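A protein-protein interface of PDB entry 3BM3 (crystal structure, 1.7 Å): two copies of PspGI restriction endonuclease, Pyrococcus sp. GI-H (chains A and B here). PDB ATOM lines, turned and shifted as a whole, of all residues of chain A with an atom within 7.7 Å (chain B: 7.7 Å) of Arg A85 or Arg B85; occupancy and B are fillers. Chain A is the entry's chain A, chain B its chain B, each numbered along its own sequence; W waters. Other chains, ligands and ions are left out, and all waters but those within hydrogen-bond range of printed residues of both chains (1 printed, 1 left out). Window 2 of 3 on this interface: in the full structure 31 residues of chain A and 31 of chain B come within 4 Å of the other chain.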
ATOM      1  N   ARG A  75      -0.775   3.416 -10.153  1.00  0.00           N
ATOM      2  CA  ARG A  75      -0.313   3.229 -11.514  1.00  0.00           C
ATOM      3  C   ARG A  75      -0.836   1.925 -12.098  1.00  0.00           C
ATOM      4  O   ARG A  75      -1.431   1.880 -13.197  1.00  0.00           O
ATOM      5  CB  ARG A  75       1.216   3.220 -11.548  1.00  0.00           C
ATOM      6  CG  ARG A  75       1.740   3.090 -12.977  1.00  0.00           C
ATOM      7  CD  ARG A  75       3.249   3.065 -13.005  1.00  0.00           C
ATOM      8  NE  ARG A  75       3.783   4.389 -12.750  1.00  0.00           N
ATOM      9  CZ  ARG A  75       4.338   4.799 -11.615  1.00  0.00           C
ATOM     10  NH1 ARG A  75       4.475   3.976 -10.582  1.00  0.00           N
ATOM     11  NH2 ARG A  75       4.759   6.037 -11.517  1.00  0.00           N
ATOM     12  N   TYR A  78      -4.585   2.079 -12.833  1.00  0.00           N
ATOM     13  CA  TYR A  78      -4.918   2.918 -13.990  1.00  0.00           C
ATOM     14  C   TYR A  78      -4.425   2.307 -15.296  1.00  0.00           C
ATOM     15  O   TYR A  78      -5.091   2.420 -16.310  1.00  0.00           O
ATOM     16  CB  TYR A  78      -4.454   4.357 -13.814  1.00  0.00           C
ATOM     17  CG  TYR A  78      -5.425   5.110 -12.964  1.00  0.00           C
ATOM     18  CD1 TYR A  78      -5.439   4.943 -11.581  1.00  0.00           C
ATOM     19  CD2 TYR A  78      -6.361   5.969 -13.524  1.00  0.00           C
ATOM     20  CE1 TYR A  78      -6.351   5.619 -10.787  1.00  0.00           C
ATOM     21  CE2 TYR A  78      -7.280   6.670 -12.728  1.00  0.00           C
ATOM     22  CZ  TYR A  78      -7.269   6.479 -11.359  1.00  0.00           C
ATOM     23  OH  TYR A  78      -8.167   7.142 -10.552  1.00  0.00           O
ATOM     24  N   LEU A  79      -3.287   1.632 -15.268  1.00  0.00           N
ATOM     25  CA  LEU A  79      -2.801   0.974 -16.489  1.00  0.00           C
ATOM     26  C   LEU A  79      -3.753  -0.161 -16.836  1.00  0.00           C
ATOM     27  O   LEU A  79      -4.080  -0.370 -18.021  1.00  0.00           O
ATOM     28  CB  LEU A  79      -1.385   0.440 -16.311  1.00  0.00           C
ATOM     29  CG  LEU A  79      -0.311   1.510 -16.110  1.00  0.00           C
ATOM     30  CD1 LEU A  79       1.083   0.847 -16.169  1.00  0.00           C
ATOM     31  CD2 LEU A  79      -0.440   2.651 -17.052  1.00  0.00           C
ATOM     32  N   GLY A  82      -6.518   1.093 -18.780  1.00  0.00           N
ATOM     33  CA  GLY A  82      -6.226   1.695 -20.084  1.00  0.00           C
ATOM     34  C   GLY A  82      -6.059   3.206 -20.081  1.00  0.00           C
ATOM     35  O   GLY A  82      -6.071   3.857 -21.137  1.00  0.00           O
ATOM     36  N   TYR A  83      -5.804   3.777 -18.901  1.00  0.00           N
ATOM     37  CA  TYR A  83      -5.631   5.207 -18.761  1.00  0.00           C
ATOM     38  C   TYR A  83      -4.377   5.731 -19.479  1.00  0.00           C
ATOM     39  O   TYR A  83      -3.363   5.072 -19.495  1.00  0.00           O
ATOM     40  CB  TYR A  83      -5.553   5.525 -17.287  1.00  0.00           C
ATOM     41  CG  TYR A  83      -5.708   6.963 -16.937  1.00  0.00           C
ATOM     42  CD1 TYR A  83      -6.948   7.478 -16.616  1.00  0.00           C
ATOM     43  CD2 TYR A  83      -4.608   7.786 -16.820  1.00  0.00           C
ATOM     44  CE1 TYR A  83      -7.084   8.786 -16.235  1.00  0.00           C
ATOM     45  CE2 TYR A  83      -4.734   9.092 -16.478  1.00  0.00           C
ATOM     46  CZ  TYR A  83      -5.973   9.586 -16.172  1.00  0.00           C
ATOM     47  OH  TYR A  83      -6.142  10.885 -15.794  1.00  0.00           O
ATOM     48  N   SER A  84      -4.452   6.942 -20.017  1.00  0.00           N
ATOM     49  CA  SER A  84      -3.323   7.557 -20.741  1.00  0.00           C
ATOM     50  C   SER A  84      -2.083   7.532 -19.873  1.00  0.00           C
ATOM     51  O   SER A  84      -2.065   8.160 -18.814  1.00  0.00           O
ATOM     52  CB  SER A  84      -3.602   9.004 -21.090  1.00  0.00           C
ATOM     53  OG  SER A  84      -2.399   9.658 -21.474  1.00  0.00           O
ATOM     54  N   ARG A  85      -1.063   6.818 -20.319  1.00  0.00           N
ATOM     55  CA  ARG A  85       0.174   6.726 -19.538  1.00  0.00           C
ATOM     56  C   ARG A  85       0.869   8.062 -19.388  1.00  0.00           C
ATOM     57  O   ARG A  85       1.416   8.359 -18.333  1.00  0.00           O
ATOM     58  CB  ARG A  85       1.141   5.756 -20.192  1.00  0.00           C
ATOM     59  CG  ARG A  85       2.379   5.470 -19.360  1.00  0.00           C
ATOM     60  CD  ARG A  85       2.019   4.783 -18.066  1.00  0.00           C
ATOM     61  NE  ARG A  85       3.150   4.533 -17.204  1.00  0.00           N
ATOM     62  CZ  ARG A  85       3.896   3.429 -17.141  1.00  0.00           C
ATOM     63  NH1 ARG A  85       4.882   3.379 -16.280  1.00  0.00           N
ATOM     64  NH2 ARG A  85       3.681   2.385 -17.935  1.00  0.00           N
ATOM     65  N   GLU A  86       0.902   8.825 -20.475  1.00  0.00           N
ATOM     66  CA  GLU A  86       1.520  10.131 -20.460  1.00  0.00           C
ATOM     67  C   GLU A  86       0.805  11.015 -19.431  1.00  0.00           C
ATOM     68  O   GLU A  86       1.439  11.711 -18.653  1.00  0.00           O
ATOM     69  CB  GLU A  86       1.428  10.773 -21.822  1.00  0.00           C
ATOM     70  CG  GLU A  86       2.265  10.070 -22.852  1.00  0.00           C
ATOM     71  CD  GLU A  86       1.531   8.991 -23.660  1.00  0.00           C
ATOM     72  OE1 GLU A  86       0.465   8.425 -23.222  1.00  0.00           O
ATOM     73  OE2 GLU A  86       2.077   8.696 -24.759  1.00  0.00           O
ATOM     74  N   LYS A  87      -0.520  10.981 -19.434  1.00  0.00           N
ATOM     75  CA  LYS A  87      -1.261  11.824 -18.500  1.00  0.00           C
ATOM     76  C   LYS A  87      -1.092  11.339 -17.069  1.00  0.00           C
ATOM     77  O   LYS A  87      -0.911  12.131 -16.161  1.00  0.00           O
ATOM     78  CB  LYS A  87      -2.738  11.935 -18.894  1.00  0.00           C
ATOM     79  CG  LYS A  87      -2.923  12.837 -20.133  1.00  0.00           C
ATOM     80  CD  LYS A  87      -2.198  14.232 -20.082  1.00  0.00           C
ATOM     81  CE  LYS A  87      -2.986  15.338 -19.331  1.00  0.00           C
ATOM     82  NZ  LYS A  87      -2.400  16.714 -19.498  1.00  0.00           N
ATOM     83  N   LEU A  88      -1.076  10.032 -16.898  1.00  0.00           N
ATOM     84  CA  LEU A  88      -0.885   9.433 -15.593  1.00  0.00           C
ATOM     85  C   LEU A  88       0.458   9.857 -14.994  1.00  0.00           C
ATOM     86  O   LEU A  88       0.559  10.313 -13.842  1.00  0.00           O
ATOM     87  CB  LEU A  88      -0.927   7.913 -15.763  1.00  0.00           C
ATOM     88  CG  LEU A  88      -0.824   7.129 -14.465  1.00  0.00           C
ATOM     89  CD1 LEU A  88      -1.980   7.437 -13.493  1.00  0.00           C
ATOM     90  CD2 LEU A  88      -0.840   5.642 -14.821  1.00  0.00           C
ATOM     91  N   GLU A  89       1.497   9.687 -15.783  1.00  0.00           N
ATOM     92  CA  GLU A  89       2.840  10.003 -15.308  1.00  0.00           C
ATOM     93  C   GLU A  89       3.017  11.498 -15.103  1.00  0.00           C
ATOM     94  O   GLU A  89       3.728  11.917 -14.182  1.00  0.00           O
ATOM     95  CB  GLU A  89       3.895   9.430 -16.235  1.00  0.00           C
ATOM     96  CG  GLU A  89       3.862   7.901 -16.300  1.00  0.00           C
ATOM     97  CD  GLU A  89       4.109   7.184 -15.000  1.00  0.00           C
ATOM     98  OE1 GLU A  89       4.552   7.767 -13.990  1.00  0.00           O
ATOM     99  OE2 GLU A  89       3.895   5.961 -15.005  1.00  0.00           O
ATOM    100  N   GLN A  90       2.322  12.305 -15.903  1.00  0.00           N
ATOM    101  CA  GLN A  90       2.434  13.747 -15.706  1.00  0.00           C
ATOM    102  C   GLN A  90       1.782  14.067 -14.372  1.00  0.00           C
ATOM    103  O   GLN A  90       2.312  14.833 -13.565  1.00  0.00           O
ATOM    104  CB  GLN A  90       1.718  14.503 -16.820  1.00  0.00           C
ATOM    105  CG  GLN A  90       1.753  15.978 -16.580  1.00  0.00           C
ATOM    106  CD  GLN A  90       0.890  16.727 -17.524  1.00  0.00           C
ATOM    107  OE1 GLN A  90      -0.275  16.379 -17.679  1.00  0.00           O
ATOM    108  NE2 GLN A  90       1.452  17.727 -18.181  1.00  0.00           N
ATOM    109  N   SER A  91       0.604  13.491 -14.160  1.00  0.00           N
ATOM    110  CA  SER A  91      -0.140  13.699 -12.912  1.00  0.00           C
ATOM    111  C   SER A  91       0.668  13.288 -11.699  1.00  0.00           C
ATOM    112  O   SER A  91       0.721  14.014 -10.705  1.00  0.00           O
ATOM    113  CB  SER A  91      -1.499  13.003 -12.932  1.00  0.00           C
ATOM    114  OG  SER A  91      -2.398  13.629 -13.848  1.00  0.00           O
ATOM    115  N   PHE A  92       1.363  12.161 -11.792  1.00  0.00           N
ATOM    116  CA  PHE A  92       2.190  11.734 -10.707  1.00  0.00           C
ATOM    117  C   PHE A  92       3.360  12.692 -10.480  1.00  0.00           C
ATOM    118  O   PHE A  92       3.652  12.989  -9.346  1.00  0.00           O
ATOM    119  CB  PHE A  92       2.742  10.362 -10.960  1.00  0.00           C
ATOM    120  CG  PHE A  92       1.742   9.245 -10.859  1.00  0.00           C
ATOM    121  CD1 PHE A  92       0.637   9.280 -10.009  1.00  0.00           C
ATOM    122  CD2 PHE A  92       1.950   8.106 -11.606  1.00  0.00           C
ATOM    123  CE1 PHE A  92      -0.223   8.188  -9.884  1.00  0.00           C
ATOM    124  CE2 PHE A  92       1.079   7.052 -11.503  1.00  0.00           C
ATOM    125  CZ  PHE A  92       0.013   7.076 -10.644  1.00  0.00           C
ATOM    126  N   ARG B  75       9.894   8.301 -27.775  1.00  0.00           N
ATOM    127  CA  ARG B  75       9.173   7.429 -26.855  1.00  0.00           C
ATOM    128  C   ARG B  75       9.142   6.042 -27.400  1.00  0.00           C
ATOM    129  O   ARG B  75       9.445   5.064 -26.721  1.00  0.00           O
ATOM    130  CB  ARG B  75       7.738   7.881 -26.667  1.00  0.00           C
ATOM    131  CG  ARG B  75       6.959   7.033 -25.701  1.00  0.00           C
ATOM    132  CD  ARG B  75       5.555   7.572 -25.531  1.00  0.00           C
ATOM    133  NE  ARG B  75       5.527   8.824 -24.769  1.00  0.00           N
ATOM    134  CZ  ARG B  75       5.241  10.014 -25.272  1.00  0.00           C
ATOM    135  NH1 ARG B  75       4.942  10.160 -26.565  1.00  0.00           N
ATOM    136  NH2 ARG B  75       5.255  11.066 -24.473  1.00  0.00           N
ATOM    137  N   TYR B  78      12.607   4.337 -27.462  1.00  0.00           N
ATOM    138  CA  TYR B  78      13.086   4.003 -26.138  1.00  0.00           C
ATOM    139  C   TYR B  78      12.265   2.922 -25.464  1.00  0.00           C
ATOM    140  O   TYR B  78      12.799   2.090 -24.754  1.00  0.00           O
ATOM    141  CB  TYR B  78      13.252   5.235 -25.256  1.00  0.00           C
ATOM    142  CG  TYR B  78      14.557   5.919 -25.479  1.00  0.00           C
ATOM    143  CD1 TYR B  78      14.751   6.726 -26.588  1.00  0.00           C
ATOM    144  CD2 TYR B  78      15.631   5.735 -24.615  1.00  0.00           C
ATOM    145  CE1 TYR B  78      15.978   7.346 -26.819  1.00  0.00           C
ATOM    146  CE2 TYR B  78      16.863   6.383 -24.835  1.00  0.00           C
ATOM    147  CZ  TYR B  78      17.026   7.153 -25.959  1.00  0.00           C
ATOM    148  OH  TYR B  78      18.209   7.801 -26.191  1.00  0.00           O
ATOM    149  N   LEU B  79      10.963   2.904 -25.681  1.00  0.00           N
ATOM    150  CA  LEU B  79      10.168   1.829 -25.147  1.00  0.00           C
ATOM    151  C   LEU B  79      10.521   0.514 -25.833  1.00  0.00           C
ATOM    152  O   LEU B  79      10.552  -0.522 -25.192  1.00  0.00           O
ATOM    153  CB  LEU B  79       8.698   2.141 -25.281  1.00  0.00           C
ATOM    154  CG  LEU B  79       8.304   3.273 -24.336  1.00  0.00           C
ATOM    155  CD1 LEU B  79       6.868   3.672 -24.596  1.00  0.00           C
ATOM    156  CD2 LEU B  79       8.530   2.939 -22.846  1.00  0.00           C
ATOM    157  N   GLY B  82      13.312  -0.938 -24.156  1.00  0.00           N
ATOM    158  CA  GLY B  82      13.050  -1.360 -22.774  1.00  0.00           C
ATOM    159  C   GLY B  82      13.236  -0.293 -21.716  1.00  0.00           C
ATOM    160  O   GLY B  82      13.250  -0.600 -20.529  1.00  0.00           O
ATOM    161  N   TYR B  83      13.363   0.967 -22.127  1.00  0.00           N
ATOM    162  CA  TYR B  83      13.633   2.059 -21.217  1.00  0.00           C
ATOM    163  C   TYR B  83      12.440   2.254 -20.305  1.00  0.00           C
ATOM    164  O   TYR B  83      11.286   2.103 -20.730  1.00  0.00           O
ATOM    165  CB  TYR B  83      13.905   3.309 -22.006  1.00  0.00           C
ATOM    166  CG  TYR B  83      14.579   4.397 -21.249  1.00  0.00           C
ATOM    167  CD1 TYR B  83      15.955   4.535 -21.286  1.00  0.00           C
ATOM    168  CD2 TYR B  83      13.844   5.355 -20.604  1.00  0.00           C
ATOM    169  CE1 TYR B  83      16.571   5.584 -20.640  1.00  0.00           C
ATOM    170  CE2 TYR B  83      14.440   6.366 -19.936  1.00  0.00           C
ATOM    171  CZ  TYR B  83      15.789   6.502 -19.977  1.00  0.00           C
ATOM    172  OH  TYR B  83      16.395   7.541 -19.323  1.00  0.00           O
ATOM    173  N   SER B  84      12.720   2.539 -19.034  1.00  0.00           N
ATOM    174  CA  SER B  84      11.658   2.805 -18.062  1.00  0.00           C
ATOM    175  C   SER B  84      10.639   3.822 -18.575  1.00  0.00           C
ATOM    176  O   SER B  84      11.004   4.971 -18.866  1.00  0.00           O
ATOM    177  CB  SER B  84      12.269   3.357 -16.776  1.00  0.00           C
ATOM    178  OG  SER B  84      11.258   3.871 -15.925  1.00  0.00           O
ATOM    179  N   ARG B  85       9.368   3.438 -18.611  1.00  0.00           N
ATOM    180  CA  ARG B  85       8.343   4.343 -19.087  1.00  0.00           C
ATOM    181  C   ARG B  85       8.193   5.525 -18.133  1.00  0.00           C
ATOM    182  O   ARG B  85       8.004   6.652 -18.554  1.00  0.00           O
ATOM    183  CB  ARG B  85       6.988   3.660 -19.219  1.00  0.00           C
ATOM    184  CG  ARG B  85       5.893   4.562 -19.746  1.00  0.00           C
ATOM    185  CD  ARG B  85       6.172   5.020 -21.130  1.00  0.00           C
ATOM    186  NE  ARG B  85       5.151   5.854 -21.729  1.00  0.00           N
ATOM    187  CZ  ARG B  85       4.070   5.438 -22.391  1.00  0.00           C
ATOM    188  NH1 ARG B  85       3.785   4.138 -22.520  1.00  0.00           N
ATOM    189  NH2 ARG B  85       3.257   6.352 -22.900  1.00  0.00           N
ATOM    190  N   GLU B  86       8.263   5.248 -16.834  1.00  0.00           N
ATOM    191  CA  GLU B  86       8.089   6.329 -15.884  1.00  0.00           C
ATOM    192  C   GLU B  86       9.199   7.368 -16.023  1.00  0.00           C
ATOM    193  O   GLU B  86       8.917   8.575 -16.061  1.00  0.00           O
ATOM    194  CB  GLU B  86       8.037   5.748 -14.493  1.00  0.00           C
ATOM    195  CG  GLU B  86       7.829   6.766 -13.399  1.00  0.00           C
ATOM    196  CD  GLU B  86       8.165   6.163 -12.039  1.00  0.00           C
ATOM    197  OE1 GLU B  86       7.854   4.970 -11.829  1.00  0.00           O
ATOM    198  OE2 GLU B  86       8.762   6.894 -11.198  1.00  0.00           O
ATOM    199  N   LYS B  87      10.443   6.931 -16.155  1.00  0.00           N
ATOM    200  CA  LYS B  87      11.569   7.857 -16.282  1.00  0.00           C
ATOM    201  C   LYS B  87      11.483   8.605 -17.587  1.00  0.00           C
ATOM    202  O   LYS B  87      11.794   9.783 -17.649  1.00  0.00           O
ATOM    203  CB  LYS B  87      12.911   7.148 -16.222  1.00  0.00           C
ATOM    204  CG  LYS B  87      13.242   6.614 -14.853  1.00  0.00           C
ATOM    205  CD  LYS B  87      13.086   7.646 -13.740  1.00  0.00           C
ATOM    206  CE  LYS B  87      13.309   7.003 -12.391  1.00  0.00           C
ATOM    207  NZ  LYS B  87      12.138   6.141 -12.025  1.00  0.00           N
ATOM    208  N   LEU B  88      11.103   7.890 -18.635  1.00  0.00           N
ATOM    209  CA  LEU B  88      10.967   8.478 -19.945  1.00  0.00           C
ATOM    210  C   LEU B  88       9.943   9.602 -19.883  1.00  0.00           C
ATOM    211  O   LEU B  88      10.211  10.699 -20.371  1.00  0.00           O
ATOM    212  CB  LEU B  88      10.510   7.417 -20.958  1.00  0.00           C
ATOM    213  CG  LEU B  88      10.477   7.700 -22.450  1.00  0.00           C
ATOM    214  CD1 LEU B  88      11.774   8.232 -23.019  1.00  0.00           C
ATOM    215  CD2 LEU B  88      10.094   6.376 -23.149  1.00  0.00           C
ATOM    216  N   GLU B  89       8.790   9.349 -19.267  1.00  0.00           N
ATOM    217  CA  GLU B  89       7.739  10.374 -19.228  1.00  0.00           C
ATOM    218  C   GLU B  89       8.178  11.543 -18.354  1.00  0.00           C
ATOM    219  O   GLU B  89       7.840  12.684 -18.624  1.00  0.00           O
ATOM    220  CB  GLU B  89       6.396   9.817 -18.778  1.00  0.00           C
ATOM    221  CG  GLU B  89       5.832   8.800 -19.758  1.00  0.00           C
ATOM    222  CD  GLU B  89       5.593   9.324 -21.169  1.00  0.00           C
ATOM    223  OE1 GLU B  89       5.542  10.557 -21.404  1.00  0.00           O
ATOM    224  OE2 GLU B  89       5.469   8.474 -22.064  1.00  0.00           O
ATOM    225  N   GLN B  90       8.941  11.237 -17.309  1.00  0.00           N
ATOM    226  CA  GLN B  90       9.452  12.298 -16.431  1.00  0.00           C
ATOM    227  C   GLN B  90      10.379  13.173 -17.226  1.00  0.00           C
ATOM    228  O   GLN B  90      10.290  14.415 -17.210  1.00  0.00           O
ATOM    229  CB  GLN B  90      10.221  11.722 -15.255  1.00  0.00           C
ATOM    230  CG  GLN B  90      10.772  12.834 -14.387  1.00  0.00           C
ATOM    231  CD  GLN B  90      11.666  12.328 -13.295  1.00  0.00           C
ATOM    232  OE1 GLN B  90      12.530  11.509 -13.549  1.00  0.00           O
ATOM    233  NE2 GLN B  90      11.445  12.792 -12.077  1.00  0.00           N
ATOM    234  N   SER B  91      11.280  12.526 -17.945  1.00  0.00           N
ATOM    235  CA  SER B  91      12.237  13.223 -18.799  1.00  0.00           C
ATOM    236  C   SER B  91      11.518  14.117 -19.796  1.00  0.00           C
ATOM    237  O   SER B  91      11.896  15.247 -20.022  1.00  0.00           O
ATOM    238  CB  SER B  91      13.141  12.216 -19.506  1.00  0.00           C
ATOM    239  OG  SER B  91      14.032  11.657 -18.558  1.00  0.00           O
ATOM    240  N   PHE B  92      10.486  13.586 -20.409  1.00  0.00           N
ATOM    241  CA  PHE B  92       9.732  14.333 -21.350  1.00  0.00           C
ATOM    242  C   PHE B  92       9.031  15.537 -20.720  1.00  0.00           C
ATOM    243  O   PHE B  92       9.030  16.618 -21.285  1.00  0.00           O
ATOM    244  CB  PHE B  92       8.707  13.457 -22.038  1.00  0.00           C
ATOM    245  CG  PHE B  92       9.295  12.489 -23.024  1.00  0.00           C
ATOM    246  CD1 PHE B  92      10.468  12.753 -23.740  1.00  0.00           C
ATOM    247  CD2 PHE B  92       8.612  11.302 -23.275  1.00  0.00           C
ATOM    248  CE1 PHE B  92      10.964  11.816 -24.709  1.00  0.00           C
ATOM    249  CE2 PHE B  92       9.076  10.402 -24.251  1.00  0.00           C
ATOM    250  CZ  PHE B  92      10.234  10.648 -24.948  1.00  0.00           C
HETATM  251  O   HOH W   1       5.753  12.956 -16.282  1.00  0.00           O
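NH2 of Arg A75 is in salt-bridge range of OE1 of Glu B86 (3.3 Å).
OE2 of Glu A86 is in salt-bridge range of NH2 of Arg B85.
The side-chain carboxylate (OE2) of Glu A86 is in salt-bridge range of the guanidinium group (NE) of Arg B75 (3.5 Å).
The guanidinium group (NE) of Arg B75 is in salt-bridge range of the side-chain carboxylate (OE2) of Glu B89 (2.7 Å).
The guanidinium group of Arg A75 lies within salt-bridge range of the side-chain carboxylate of Glu A89 (2.8 Å).
The guanidinium group of Arg A85 is in salt-bridge range of the side-chain carboxylate of Glu A89, at 2.7 Å.
NE of Arg B85 lies within salt-bridge range of OE2 of Glu B89 (2.7 Å).
The side-chain amino group of Lys B87 is in salt-bridge range of the side-chain carboxylate of Glu B86 (3.6 Å).
The side-chain hydroxyl of Ser B84 sits close to the backbone NH of Glu B86.
CG of Arg A85 touches CZ of Arg B85 (3.5 Å).
Glu B86 touches Arg A85.
Glu B89 touches Glu A86 (OE1 to CG, 3.6 Å).
Glu A89 touches Glu B86.
Glu A89 touches Glu B89.
Printed residues of chain B within 4 Å of Arg A75: Glu B86.
No residue of chain B comes within 4 Å of Ser A84.
Of the printed residues of chain B, Glu A86 touches Arg B75 (3.5 Å), Arg B85 (3.2 Å) and Glu B89 (3.6 Å).
Tyr B78 touches none of the printed residues of chain A.
No residue of chain A comes within 4 Å of Ser B84.
Arg B85 touches two residues of chain A.
The nearest printed residue of chain A that does not touch Glu B86 is Phe A92 (6.3 Å).
Along chain A the printed residues that touch a printed residue of chain B span positions 75 to 89.
Of the 14 printed residues of chain B, 4 touch a printed residue of chain A.
Arg B85 touches its own counterpart, Arg A85.
Arg A85 touches Glu B86, and with the chains exchanged Glu A86 touches Arg B85.
Glu A86 touches Glu B89, and with the chains exchanged Glu A89 touches Glu B86.
Glu B89 touches its own counterpart, Glu A89.
Positions printed for both chains: 75, 78, 79, 82, 83, 84, 85, 86, 87, 88, 89, 90, 91 and 92.
Water W1 bridges O of Glu A89 and O of Glu B89.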
